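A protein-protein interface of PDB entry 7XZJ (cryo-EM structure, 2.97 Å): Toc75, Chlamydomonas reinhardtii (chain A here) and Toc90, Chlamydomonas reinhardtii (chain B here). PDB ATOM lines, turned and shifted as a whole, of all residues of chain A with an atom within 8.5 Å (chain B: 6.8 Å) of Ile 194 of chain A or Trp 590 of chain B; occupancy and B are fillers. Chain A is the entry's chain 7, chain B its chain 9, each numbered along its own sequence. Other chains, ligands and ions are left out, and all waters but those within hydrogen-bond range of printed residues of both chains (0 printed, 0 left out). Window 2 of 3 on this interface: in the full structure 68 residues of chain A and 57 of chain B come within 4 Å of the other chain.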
ATOM      1  N   GLU A 156      26.681  -9.542  25.870  1.00  0.00           N
ATOM      2  CA  GLU A 156      27.276  -8.307  26.445  1.00  0.00           C
ATOM      3  C   GLU A 156      26.622  -8.032  27.802  1.00  0.00           C
ATOM      4  O   GLU A 156      25.379  -8.050  27.870  1.00  0.00           O
ATOM      5  CB  GLU A 156      27.033  -7.120  25.512  1.00  0.00           C
ATOM      6  CG  GLU A 156      27.643  -7.295  24.135  1.00  0.00           C
ATOM      7  CD  GLU A 156      27.478  -6.094  23.220  1.00  0.00           C
ATOM      8  OE1 GLU A 156      26.713  -5.179  23.580  1.00  0.00           O
ATOM      9  OE2 GLU A 156      28.121  -6.075  22.152  1.00  0.00           O
ATOM     10  N   ARG A 157      27.429  -7.749  28.828  1.00  0.00           N
ATOM     11  CA  ARG A 157      26.903  -7.453  30.190  1.00  0.00           C
ATOM     12  C   ARG A 157      27.738  -6.310  30.771  1.00  0.00           C
ATOM     13  O   ARG A 157      28.978  -6.384  30.662  1.00  0.00           O
ATOM     14  CB  ARG A 157      26.979  -8.696  31.081  1.00  0.00           C
ATOM     15  CG  ARG A 157      26.542  -8.460  32.520  1.00  0.00           C
ATOM     16  CD  ARG A 157      26.840  -9.652  33.407  1.00  0.00           C
ATOM     17  NE  ARG A 157      26.477  -9.412  34.795  1.00  0.00           N
ATOM     18  CZ  ARG A 157      26.659 -10.283  35.780  1.00  0.00           C
ATOM     19  NH1 ARG A 157      27.207 -11.460  35.528  1.00  0.00           N
ATOM     20  NH2 ARG A 157      26.297  -9.976  37.012  1.00  0.00           N
ATOM     21  N   SER A 158      27.097  -5.299  31.364  1.00  0.00           N
ATOM     22  CA  SER A 158      27.864  -4.115  31.833  1.00  0.00           C
ATOM     23  C   SER A 158      27.315  -3.619  33.170  1.00  0.00           C
ATOM     24  O   SER A 158      26.140  -3.882  33.448  1.00  0.00           O
ATOM     25  CB  SER A 158      27.824  -3.019  30.803  1.00  0.00           C
ATOM     26  OG  SER A 158      28.500  -1.862  31.270  1.00  0.00           O
ATOM     27  N   GLY A 159      28.136  -2.909  33.949  1.00  0.00           N
ATOM     28  CA  GLY A 159      27.684  -2.347  35.238  1.00  0.00           C
ATOM     29  C   GLY A 159      27.014  -0.999  35.046  1.00  0.00           C
ATOM     30  O   GLY A 159      26.549  -0.426  36.051  1.00  0.00           O
ATOM     31  N   THR A 160      26.967  -0.506  33.806  1.00  0.00           N
ATOM     32  CA  THR A 160      26.364   0.817  33.501  1.00  0.00           C
ATOM     33  C   THR A 160      24.847   0.674  33.357  1.00  0.00           C
ATOM     34  O   THR A 160      24.328  -0.425  33.628  1.00  0.00           O
ATOM     35  CB  THR A 160      26.935   1.387  32.200  1.00  0.00           C
ATOM     36  OG1 THR A 160      26.694   0.417  31.183  1.00  0.00           O
ATOM     37  CG2 THR A 160      28.417   1.681  32.287  1.00  0.00           C
ATOM     38  N   ASN A 161      24.172   1.746  32.932  1.00  0.00           N
ATOM     39  CA  ASN A 161      22.696   1.703  32.757  1.00  0.00           C
ATOM     40  C   ASN A 161      22.405   1.011  31.425  1.00  0.00           C
ATOM     41  O   ASN A 161      22.131   1.714  30.437  1.00  0.00           O
ATOM     42  CB  ASN A 161      22.057   3.090  32.883  1.00  0.00           C
ATOM     43  CG  ASN A 161      22.770   4.187  32.119  1.00  0.00           C
ATOM     44  OD1 ASN A 161      23.803   3.959  31.494  1.00  0.00           O
ATOM     45  ND2 ASN A 161      22.221   5.388  32.164  1.00  0.00           N
ATOM     46  N   ARG A 162      22.436  -0.324  31.419  1.00  0.00           N
ATOM     47  CA  ARG A 162      22.267  -1.086  30.155  1.00  0.00           C
ATOM     48  C   ARG A 162      20.865  -1.695  30.111  1.00  0.00           C
ATOM     49  O   ARG A 162      20.505  -2.409  31.063  1.00  0.00           O
ATOM     50  CB  ARG A 162      23.340  -2.176  30.100  1.00  0.00           C
ATOM     51  CG  ARG A 162      23.371  -2.972  28.805  1.00  0.00           C
ATOM     52  CD  ARG A 162      24.434  -4.050  28.882  1.00  0.00           C
ATOM     53  NE  ARG A 162      24.295  -4.831  30.102  1.00  0.00           N
ATOM     54  CZ  ARG A 162      23.605  -5.960  30.204  1.00  0.00           C
ATOM     55  NH1 ARG A 162      22.988  -6.460  29.148  1.00  0.00           N
ATOM     56  NH2 ARG A 162      23.541  -6.592  31.362  1.00  0.00           N
ATOM     57  N   CYS A 163      20.118  -1.431  29.036  1.00  0.00           N
ATOM     58  CA  CYS A 163      18.737  -1.962  28.892  1.00  0.00           C
ATOM     59  C   CYS A 163      18.760  -3.491  28.876  1.00  0.00           C
ATOM     60  O   CYS A 163      19.566  -4.056  28.121  1.00  0.00           O
ATOM     61  CB  CYS A 163      18.101  -1.464  27.602  1.00  0.00           C
ATOM     62  SG  CYS A 163      16.494  -2.222  27.258  1.00  0.00           S
ATOM     63  N   VAL A 164      17.906  -4.126  29.680  1.00  0.00           N
ATOM     64  CA  VAL A 164      17.824  -5.580  29.713  1.00  0.00           C
ATOM     65  C   VAL A 164      16.675  -6.103  28.858  1.00  0.00           C
ATOM     66  O   VAL A 164      16.831  -7.098  28.150  1.00  0.00           O
ATOM     67  CB  VAL A 164      17.705  -6.075  31.170  1.00  0.00           C
ATOM     68  CG1 VAL A 164      17.165  -7.491  31.215  1.00  0.00           C
ATOM     69  CG2 VAL A 164      19.057  -6.019  31.848  1.00  0.00           C
ATOM     70  N   THR A 188      15.371   3.272  19.033  1.00  0.00           N
ATOM     71  CA  THR A 188      16.821   3.550  19.189  1.00  0.00           C
ATOM     72  C   THR A 188      17.364   2.662  20.307  1.00  0.00           C
ATOM     73  O   THR A 188      18.427   2.048  20.114  1.00  0.00           O
ATOM     74  CB  THR A 188      17.060   5.022  19.537  1.00  0.00           C
ATOM     75  OG1 THR A 188      16.503   5.260  20.829  1.00  0.00           O
ATOM     76  CG2 THR A 188      16.443   5.969  18.532  1.00  0.00           C
ATOM     77  N   VAL A 189      16.643   2.598  21.427  1.00  0.00           N
ATOM     78  CA  VAL A 189      17.084   1.765  22.536  1.00  0.00           C
ATOM     79  C   VAL A 189      17.147   0.313  22.090  1.00  0.00           C
ATOM     80  O   VAL A 189      16.245  -0.192  21.408  1.00  0.00           O
ATOM     81  CB  VAL A 189      16.143   1.936  23.739  1.00  0.00           C
ATOM     82  CG1 VAL A 189      16.595   1.068  24.902  1.00  0.00           C
ATOM     83  CG2 VAL A 189      16.074   3.399  24.153  1.00  0.00           C
ATOM     84  N   GLN A 190      18.222  -0.379  22.471  1.00  0.00           N
ATOM     85  CA  GLN A 190      18.337  -1.822  22.132  1.00  0.00           C
ATOM     86  C   GLN A 190      18.735  -2.621  23.373  1.00  0.00           C
ATOM     87  O   GLN A 190      19.427  -2.061  24.241  1.00  0.00           O
ATOM     88  CB  GLN A 190      19.339  -2.041  20.999  1.00  0.00           C
ATOM     89  CG  GLN A 190      18.800  -1.668  19.627  1.00  0.00           C
ATOM     90  CD  GLN A 190      17.600  -2.495  19.234  1.00  0.00           C
ATOM     91  OE1 GLN A 190      16.611  -1.981  18.717  1.00  0.00           O
ATOM     92  NE2 GLN A 190      17.678  -3.794  19.479  1.00  0.00           N
ATOM     93  N   GLU A 191      18.304  -3.881  23.445  1.00  0.00           N
ATOM     94  CA  GLU A 191      18.673  -4.752  24.590  1.00  0.00           C
ATOM     95  C   GLU A 191      20.183  -4.991  24.553  1.00  0.00           C
ATOM     96  O   GLU A 191      20.725  -5.154  23.444  1.00  0.00           O
ATOM     97  CB  GLU A 191      17.920  -6.079  24.518  1.00  0.00           C
ATOM     98  CG  GLU A 191      16.417  -5.941  24.684  1.00  0.00           C
ATOM     99  CD  GLU A 191      15.621  -5.883  23.391  1.00  0.00           C
ATOM    100  OE1 GLU A 191      16.234  -5.666  22.327  1.00  0.00           O
ATOM    101  OE2 GLU A 191      14.390  -6.067  23.451  1.00  0.00           O
ATOM    102  N   GLY A 192      20.829  -5.027  25.721  1.00  0.00           N
ATOM    103  CA  GLY A 192      22.285  -5.253  25.787  1.00  0.00           C
ATOM    104  C   GLY A 192      23.052  -4.003  25.404  1.00  0.00           C
ATOM    105  O   GLY A 192      24.262  -4.112  25.137  1.00  0.00           O
ATOM    106  N   HIS A 193      22.372  -2.854  25.378  1.00  0.00           N
ATOM    107  CA  HIS A 193      23.031  -1.576  25.000  1.00  0.00           C
ATOM    108  C   HIS A 193      22.696  -0.489  26.021  1.00  0.00           C
ATOM    109  O   HIS A 193      21.590  -0.536  26.585  1.00  0.00           O
ATOM    110  CB  HIS A 193      22.646  -1.175  23.574  1.00  0.00           C
ATOM    111  CG  HIS A 193      23.308  -2.008  22.530  1.00  0.00           C
ATOM    112  ND1 HIS A 193      24.677  -2.010  22.354  1.00  0.00           N
ATOM    113  CD2 HIS A 193      22.805  -2.862  21.615  1.00  0.00           C
ATOM    114  CE1 HIS A 193      24.988  -2.830  21.373  1.00  0.00           C
ATOM    115  NE2 HIS A 193      23.856  -3.364  20.902  1.00  0.00           N
ATOM    116  N   ILE A 194      23.612   0.457  26.236  1.00  0.00           N
ATOM    117  CA  ILE A 194      23.390   1.501  27.280  1.00  0.00           C
ATOM    118  C   ILE A 194      22.551   2.638  26.700  1.00  0.00           C
ATOM    119  O   ILE A 194      22.480   2.737  25.469  1.00  0.00           O
ATOM    120  CB  ILE A 194      24.721   1.994  27.878  1.00  0.00           C
ATOM    121  CG1 ILE A 194      25.368   3.098  27.039  1.00  0.00           C
ATOM    122  CG2 ILE A 194      25.662   0.824  28.106  1.00  0.00           C
ATOM    123  CD1 ILE A 194      26.400   3.899  27.796  1.00  0.00           C
ATOM    124  N   PHE A 195      21.933   3.407  27.597  1.00  0.00           N
ATOM    125  CA  PHE A 195      21.036   4.495  27.155  1.00  0.00           C
ATOM    126  C   PHE A 195      21.120   5.664  28.128  1.00  0.00           C
ATOM    127  O   PHE A 195      21.723   5.509  29.206  1.00  0.00           O
ATOM    128  CB  PHE A 195      19.594   3.985  27.055  1.00  0.00           C
ATOM    129  CG  PHE A 195      18.991   3.491  28.346  1.00  0.00           C
ATOM    130  CD1 PHE A 195      19.176   2.184  28.765  1.00  0.00           C
ATOM    131  CD2 PHE A 195      18.221   4.330  29.137  1.00  0.00           C
ATOM    132  CE1 PHE A 195      18.621   1.731  29.951  1.00  0.00           C
ATOM    133  CE2 PHE A 195      17.664   3.876  30.323  1.00  0.00           C
ATOM    134  CZ  PHE A 195      17.864   2.577  30.726  1.00  0.00           C
ATOM    135  N   GLU A 196      20.543   6.796  27.746  1.00  0.00           N
ATOM    136  CA  GLU A 196      20.494   7.986  28.576  1.00  0.00           C
ATOM    137  C   GLU A 196      19.095   8.574  28.482  1.00  0.00           C
ATOM    138  O   GLU A 196      18.255   8.112  27.706  1.00  0.00           O
ATOM    139  CB  GLU A 196      21.553   9.009  28.149  1.00  0.00           C
ATOM    140  CG  GLU A 196      21.512   9.356  26.673  1.00  0.00           C
ATOM    141  CD  GLU A 196      22.756  10.092  26.213  1.00  0.00           C
ATOM    142  OE1 GLU A 196      23.501  10.594  27.078  1.00  0.00           O
ATOM    143  OE2 GLU A 196      22.994  10.162  24.989  1.00  0.00           O
ATOM    144  N   LYS A 197      18.841   9.597  29.300  1.00  0.00           N
ATOM    145  CA  LYS A 197      17.549  10.275  29.260  1.00  0.00           C
ATOM    146  C   LYS A 197      17.247  10.822  27.871  1.00  0.00           C
ATOM    147  O   LYS A 197      16.084  10.845  27.446  1.00  0.00           O
ATOM    148  CB  LYS A 197      17.516  11.401  30.293  1.00  0.00           C
ATOM    149  CG  LYS A 197      16.168  12.081  30.436  1.00  0.00           C
ATOM    150  CD  LYS A 197      16.318  13.450  31.078  1.00  0.00           C
ATOM    151  CE  LYS A 197      17.069  13.366  32.397  1.00  0.00           C
ATOM    152  NZ  LYS A 197      17.094  14.679  33.098  1.00  0.00           N
ATOM    153  N   GLN A 198      18.281  11.255  27.148  1.00  0.00           N
ATOM    154  CA  GLN A 198      18.082  11.813  25.815  1.00  0.00           C
ATOM    155  C   GLN A 198      17.488  10.781  24.868  1.00  0.00           C
ATOM    156  O   GLN A 198      16.643  11.113  24.027  1.00  0.00           O
ATOM    157  CB  GLN A 198      19.407  12.345  25.273  1.00  0.00           C
ATOM    158  CG  GLN A 198      19.341  12.837  23.838  1.00  0.00           C
ATOM    159  CD  GLN A 198      18.413  14.020  23.674  1.00  0.00           C
ATOM    160  OE1 GLN A 198      17.570  14.045  22.777  1.00  0.00           O
ATOM    161  NE2 GLN A 198      18.565  15.014  24.540  1.00  0.00           N
ATOM    162  N   ASP A 199      17.935   9.534  25.006  1.00  0.00           N
ATOM    163  CA  ASP A 199      17.425   8.452  24.126  1.00  0.00           C
ATOM    164  C   ASP A 199      15.904   8.387  24.268  1.00  0.00           C
ATOM    165  O   ASP A 199      15.208   8.500  23.246  1.00  0.00           O
ATOM    166  CB  ASP A 199      18.114   7.127  24.450  1.00  0.00           C
ATOM    167  CG  ASP A 199      19.626   7.224  24.346  1.00  0.00           C
ATOM    168  OD1 ASP A 199      20.112   8.266  23.864  1.00  0.00           O
ATOM    169  OD2 ASP A 199      20.303   6.265  24.750  1.00  0.00           O
ATOM    170  N   ASN A 230      21.876  -1.489  38.305  1.00  0.00           N
ATOM    171  CA  ASN A 230      21.783  -0.300  37.408  1.00  0.00           C
ATOM    172  C   ASN A 230      21.189  -0.775  36.078  1.00  0.00           C
ATOM    173  O   ASN A 230      20.859   0.089  35.248  1.00  0.00           O
ATOM    174  CB  ASN A 230      23.056   0.547  37.308  1.00  0.00           C
ATOM    175  CG  ASN A 230      23.381   1.272  38.596  1.00  0.00           C
ATOM    176  OD1 ASN A 230      22.723   1.067  39.613  1.00  0.00           O
ATOM    177  ND2 ASN A 230      24.395   2.122  38.561  1.00  0.00           N
ATOM    178  N   HIS A 231      21.058  -2.096  35.889  1.00  0.00           N
ATOM    179  CA  HIS A 231      20.372  -2.620  34.678  1.00  0.00           C
ATOM    180  C   HIS A 231      18.901  -2.204  34.761  1.00  0.00           C
ATOM    181  O   HIS A 231      18.336  -2.294  35.865  1.00  0.00           O
ATOM    182  CB  HIS A 231      20.429  -4.149  34.629  1.00  0.00           C
ATOM    183  CG  HIS A 231      21.795  -4.741  34.662  1.00  0.00           C
ATOM    184  ND1 HIS A 231      22.013  -6.038  35.082  1.00  0.00           N
ATOM    185  CD2 HIS A 231      23.002  -4.241  34.328  1.00  0.00           C
ATOM    186  CE1 HIS A 231      23.297  -6.312  35.010  1.00  0.00           C
ATOM    187  NE2 HIS A 231      23.925  -5.225  34.553  1.00  0.00           N
ATOM    188  N   VAL A 234      12.899  -0.970  29.768  1.00  0.00           N
ATOM    189  CA  VAL A 234      12.187   0.193  29.161  1.00  0.00           C
ATOM    190  C   VAL A 234      10.768  -0.225  28.765  1.00  0.00           C
ATOM    191  O   VAL A 234      10.637  -1.119  27.911  1.00  0.00           O
ATOM    192  CB  VAL A 234      12.973   0.790  27.979  1.00  0.00           C
ATOM    193  CG1 VAL A 234      12.479   2.186  27.642  1.00  0.00           C
ATOM    194  CG2 VAL A 234      14.466   0.822  28.266  1.00  0.00           C
ATOM    195  N   TYR B 576      34.413   7.535  10.218  1.00  0.00           N
ATOM    196  CA  TYR B 576      33.678   7.485  11.510  1.00  0.00           C
ATOM    197  C   TYR B 576      33.338   6.036  11.858  1.00  0.00           C
ATOM    198  O   TYR B 576      33.687   5.597  12.962  1.00  0.00           O
ATOM    199  CB  TYR B 576      32.405   8.330  11.435  1.00  0.00           C
ATOM    200  CG  TYR B 576      31.524   8.285  12.657  1.00  0.00           C
ATOM    201  CD1 TYR B 576      31.828   9.032  13.785  1.00  0.00           C
ATOM    202  CD2 TYR B 576      30.375   7.513  12.683  1.00  0.00           C
ATOM    203  CE1 TYR B 576      31.020   9.002  14.909  1.00  0.00           C
ATOM    204  CE2 TYR B 576      29.561   7.467  13.802  1.00  0.00           C
ATOM    205  CZ  TYR B 576      29.882   8.218  14.917  1.00  0.00           C
ATOM    206  OH  TYR B 576      29.082   8.183  16.022  1.00  0.00           O
ATOM    207  N   MET B 580      34.629   3.996  14.961  1.00  0.00           N
ATOM    208  CA  MET B 580      33.706   3.474  15.998  1.00  0.00           C
ATOM    209  C   MET B 580      33.947   1.974  16.123  1.00  0.00           C
ATOM    210  O   MET B 580      33.968   1.483  17.257  1.00  0.00           O
ATOM    211  CB  MET B 580      32.238   3.728  15.648  1.00  0.00           C
ATOM    212  CG  MET B 580      31.872   5.193  15.627  1.00  0.00           C
ATOM    213  SD  MET B 580      32.454   6.070  17.096  1.00  0.00           S
ATOM    214  CE  MET B 580      31.033   5.892  18.173  1.00  0.00           C
ATOM    215  N   ALA B 584      35.010   0.152  19.378  1.00  0.00           N
ATOM    216  CA  ALA B 584      34.129  -0.894  19.877  1.00  0.00           C
ATOM    217  C   ALA B 584      34.842  -2.228  20.023  1.00  0.00           C
ATOM    218  O   ALA B 584      34.327  -3.116  20.709  1.00  0.00           O
ATOM    219  CB  ALA B 584      32.918  -1.046  18.958  1.00  0.00           C
ATOM    220  N   ASP B 588      34.019  -0.068  24.870  1.00  0.00           N
ATOM    221  CA  ASP B 588      33.386   1.240  24.959  1.00  0.00           C
ATOM    222  C   ASP B 588      31.917   1.111  24.597  1.00  0.00           C
ATOM    223  O   ASP B 588      31.602   0.748  23.454  1.00  0.00           O
ATOM    224  CB  ASP B 588      34.075   2.237  24.039  1.00  0.00           C
ATOM    225  CG  ASP B 588      33.586   3.658  24.249  1.00  0.00           C
ATOM    226  OD1 ASP B 588      32.384   3.919  24.032  1.00  0.00           O
ATOM    227  OD2 ASP B 588      34.402   4.516  24.644  1.00  0.00           O
ATOM    228  N   PRO B 589      30.973   1.338  25.541  1.00  0.00           N
ATOM    229  CA  PRO B 589      29.553   1.108  25.266  1.00  0.00           C
ATOM    230  C   PRO B 589      29.014   1.953  24.107  1.00  0.00           C
ATOM    231  O   PRO B 589      28.518   1.377  23.164  1.00  0.00           O
ATOM    232  CB  PRO B 589      28.858   1.548  26.560  1.00  0.00           C
ATOM    233  CG  PRO B 589      29.916   1.396  27.619  1.00  0.00           C
ATOM    234  CD  PRO B 589      31.185   1.821  26.915  1.00  0.00           C
ATOM    235  N   TRP B 590      29.115   3.279  24.206  1.00  0.00           N
ATOM    236  CA  TRP B 590      28.511   4.133  23.150  1.00  0.00           C
ATOM    237  C   TRP B 590      29.018   3.678  21.779  1.00  0.00           C
ATOM    238  O   TRP B 590      28.197   3.587  20.846  1.00  0.00           O
ATOM    239  CB  TRP B 590      28.800   5.616  23.407  1.00  0.00           C
ATOM    240  CG  TRP B 590      28.005   6.201  24.534  1.00  0.00           C
ATOM    241  CD1 TRP B 590      28.492   6.829  25.641  1.00  0.00           C
ATOM    242  CD2 TRP B 590      26.571   6.211  24.667  1.00  0.00           C
ATOM    243  NE1 TRP B 590      27.466   7.234  26.451  1.00  0.00           N
ATOM    244  CE2 TRP B 590      26.275   6.869  25.881  1.00  0.00           C
ATOM    245  CE3 TRP B 590      25.513   5.733  23.888  1.00  0.00           C
ATOM    246  CZ2 TRP B 590      24.968   7.054  26.328  1.00  0.00           C
ATOM    247  CZ3 TRP B 590      24.223   5.919  24.331  1.00  0.00           C
ATOM    248  CH2 TRP B 590      23.955   6.571  25.534  1.00  0.00           C
ATOM    249  N   ALA B 591      30.313   3.376  21.673  1.00  0.00           N
ATOM    250  CA  ALA B 591      30.878   2.892  20.393  1.00  0.00           C
ATOM    251  C   ALA B 591      30.186   1.587  20.002  1.00  0.00           C
ATOM    252  O   ALA B 591      29.701   1.490  18.861  1.00  0.00           O
ATOM    253  CB  ALA B 591      32.364   2.693  20.531  1.00  0.00           C
ATOM    254  N   GLN B 592      30.129   0.632  20.931  1.00  0.00           N
ATOM    255  CA  GLN B 592      29.512  -0.682  20.625  1.00  0.00           C
ATOM    256  C   GLN B 592      28.094  -0.446  20.106  1.00  0.00           C
ATOM    257  O   GLN B 592      27.733  -1.053  19.081  1.00  0.00           O
ATOM    258  CB  GLN B 592      29.519  -1.560  21.873  1.00  0.00           C
ATOM    259  CG  GLN B 592      30.916  -1.995  22.288  1.00  0.00           C
ATOM    260  CD  GLN B 592      30.991  -2.291  23.765  1.00  0.00           C
ATOM    261  OE1 GLN B 592      30.026  -2.114  24.502  1.00  0.00           O
ATOM    262  NE2 GLN B 592      32.152  -2.743  24.208  1.00  0.00           N
ATOM    263  N   ARG B 593      27.344   0.455  20.743  1.00  0.00           N
ATOM    264  CA  ARG B 593      25.933   0.691  20.336  1.00  0.00           C
ATOM    265  C   ARG B 593      25.879   1.305  18.933  1.00  0.00           C
ATOM    266  O   ARG B 593      25.044   0.854  18.130  1.00  0.00           O
ATOM    267  CB  ARG B 593      25.193   1.577  21.341  1.00  0.00           C
ATOM    268  CG  ARG B 593      23.683   1.538  21.163  1.00  0.00           C
ATOM    269  CD  ARG B 593      22.894   2.386  22.138  1.00  0.00           C
ATOM    270  NE  ARG B 593      22.789   3.773  21.715  1.00  0.00           N
ATOM    271  CZ  ARG B 593      21.859   4.611  22.154  1.00  0.00           C
ATOM    272  NH1 ARG B 593      20.953   4.190  23.019  1.00  0.00           N
ATOM    273  NH2 ARG B 593      21.830   5.858  21.720  1.00  0.00           N
ATOM    274  N   GLU B 594      26.726   2.297  18.648  1.00  0.00           N
ATOM    275  CA  GLU B 594      26.668   2.988  17.332  1.00  0.00           C
ATOM    276  C   GLU B 594      26.978   1.981  16.221  1.00  0.00           C
ATOM    277  O   GLU B 594      26.297   2.024  15.180  1.00  0.00           O
ATOM    278  CB  GLU B 594      27.671   4.140  17.299  1.00  0.00           C
ATOM    279  CG  GLU B 594      27.192   5.334  16.496  1.00  0.00           C
ATOM    280  CD  GLU B 594      26.310   6.298  17.269  1.00  0.00           C
ATOM    281  OE1 GLU B 594      25.720   7.194  16.636  1.00  0.00           O
ATOM    282  OE2 GLU B 594      26.223   6.156  18.506  1.00  0.00           O
ATOM    283  N   TYR B 595      27.962   1.108  16.443  1.00  0.00           N
ATOM    284  CA  TYR B 595      28.341   0.085  15.437  1.00  0.00           C
ATOM    285  C   TYR B 595      27.175  -0.889  15.249  1.00  0.00           C
ATOM    286  O   TYR B 595      26.916  -1.290  14.103  1.00  0.00           O
ATOM    287  CB  TYR B 595      29.610  -0.633  15.902  1.00  0.00           C
ATOM    288  CG  TYR B 595      30.125  -1.721  14.996  1.00  0.00           C
ATOM    289  CD1 TYR B 595      30.562  -1.439  13.713  1.00  0.00           C
ATOM    290  CD2 TYR B 595      30.212  -3.031  15.436  1.00  0.00           C
ATOM    291  CE1 TYR B 595      31.047  -2.433  12.882  1.00  0.00           C
ATOM    292  CE2 TYR B 595      30.698  -4.036  14.619  1.00  0.00           C
ATOM    293  CZ  TYR B 595      31.115  -3.738  13.336  1.00  0.00           C
ATOM    294  OH  TYR B 595      31.595  -4.724  12.523  1.00  0.00           O
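The side-chain carboxylate of Asp 199 of chain A lies within salt-bridge range of the guanidinium group of Arg 593 of chain B (2.8 Å).
O of Ile 194 of chain A lies within hydrogen-bond range of NH1 of Arg 593 of chain B (3.2 Å).
Of the printed residues of chain B, His 193 of chain A touches Gln 592 (3.99 Å) and Arg 593 (3.6 Å).
Of chain B, only Pro 589, Trp 590 and Arg 593 come within 4 Å of Ile 194 of chain A.
Printed residues of chain B within 4 Å of Phe 195 of chain A: Trp 590 (3.9 Å).
Of the printed residues of chain B, Glu 196 of chain A touches Trp 590 (3.8 Å).
Printed residues of chain B within 4 Å of Asp 199 of chain A: Trp 590 (3.7 Å) and Arg 593 (2.8 Å).
Pro 589 of chain B touches just one residue of chain A: Ile 194.
Trp 590 of chain B touches four residues of chain A.
No residue of chain A comes within 4 Å of Ala 591 of chain B.
Of the printed residues of chain A, Gln 592 of chain B touches His 193 (3.99 Å).
The nearest printed residue of chain B that does not touch Asp 199 of chain A is Glu 594 of chain B (8.4 Å).
OD2 of Asp 199 of chain A sits at hydrogen-bond distance from N of Glu 196 of chain A (3.1 Å).
The backbone carbonyl oxygen of Phe 195 of chain A sits at hydrogen-bond distance from the side-chain amide nitrogen of Asn 161 of chain A (3.0 Å).
The side-chain carboxylate (OD1) of Asp 588 of chain B lies within hydrogen-bond range of the backbone NH (N) of Trp 590 of chain B, at 3.3 Å.
The backbone carbonyl oxygen (O) of His 193 of chain A lies within hydrogen-bond range of the backbone NH (N) of Cys 163 of chain A (3.0 Å).
N of Asp 588 of chain B lies close to NE2 of Gln 592 of chain B, at 3.3 Å.
His 193 of chain A touches Gln 592 of chain B.
CA of Arg 593 of chain B touches ND1 of His 193 of chain A, 3.6 Å away.
Ile 194 of chain A touches Pro 589 of chain B (CD1 to CB, 3.6 Å).
Ile 194 of chain A touches Trp 590 of chain B (CD1 to CE2, 3.5 Å).
Phe 195 of chain A touches Trp 590 of chain B.
Glu 196 of chain A touches Trp 590 of chain B.
OD2 of Asp 199 of chain A touches CH2 of Trp 590 of chain B, at 3.7 Å.
Printed residues of chain A that touch a printed residue of chain B: His 193, Ile 194, Phe 195, Glu 196 and Asp 199.
Hydrophobic or aromatic side chains of chain A within 4 Å of the printed part of chain B: His 193 and Ile 194.
Hydrophobic or aromatic side chains of chain B within 4 Å of the printed part of chain A: Pro 589 and Trp 590.
Among the printed residues, Asp or Glu carboxylates within 4 Å of a Lys or Arg side-chain nitrogen of the other chain: Asp 199 of chain A with Arg 593 of chain B (2.8 Å).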
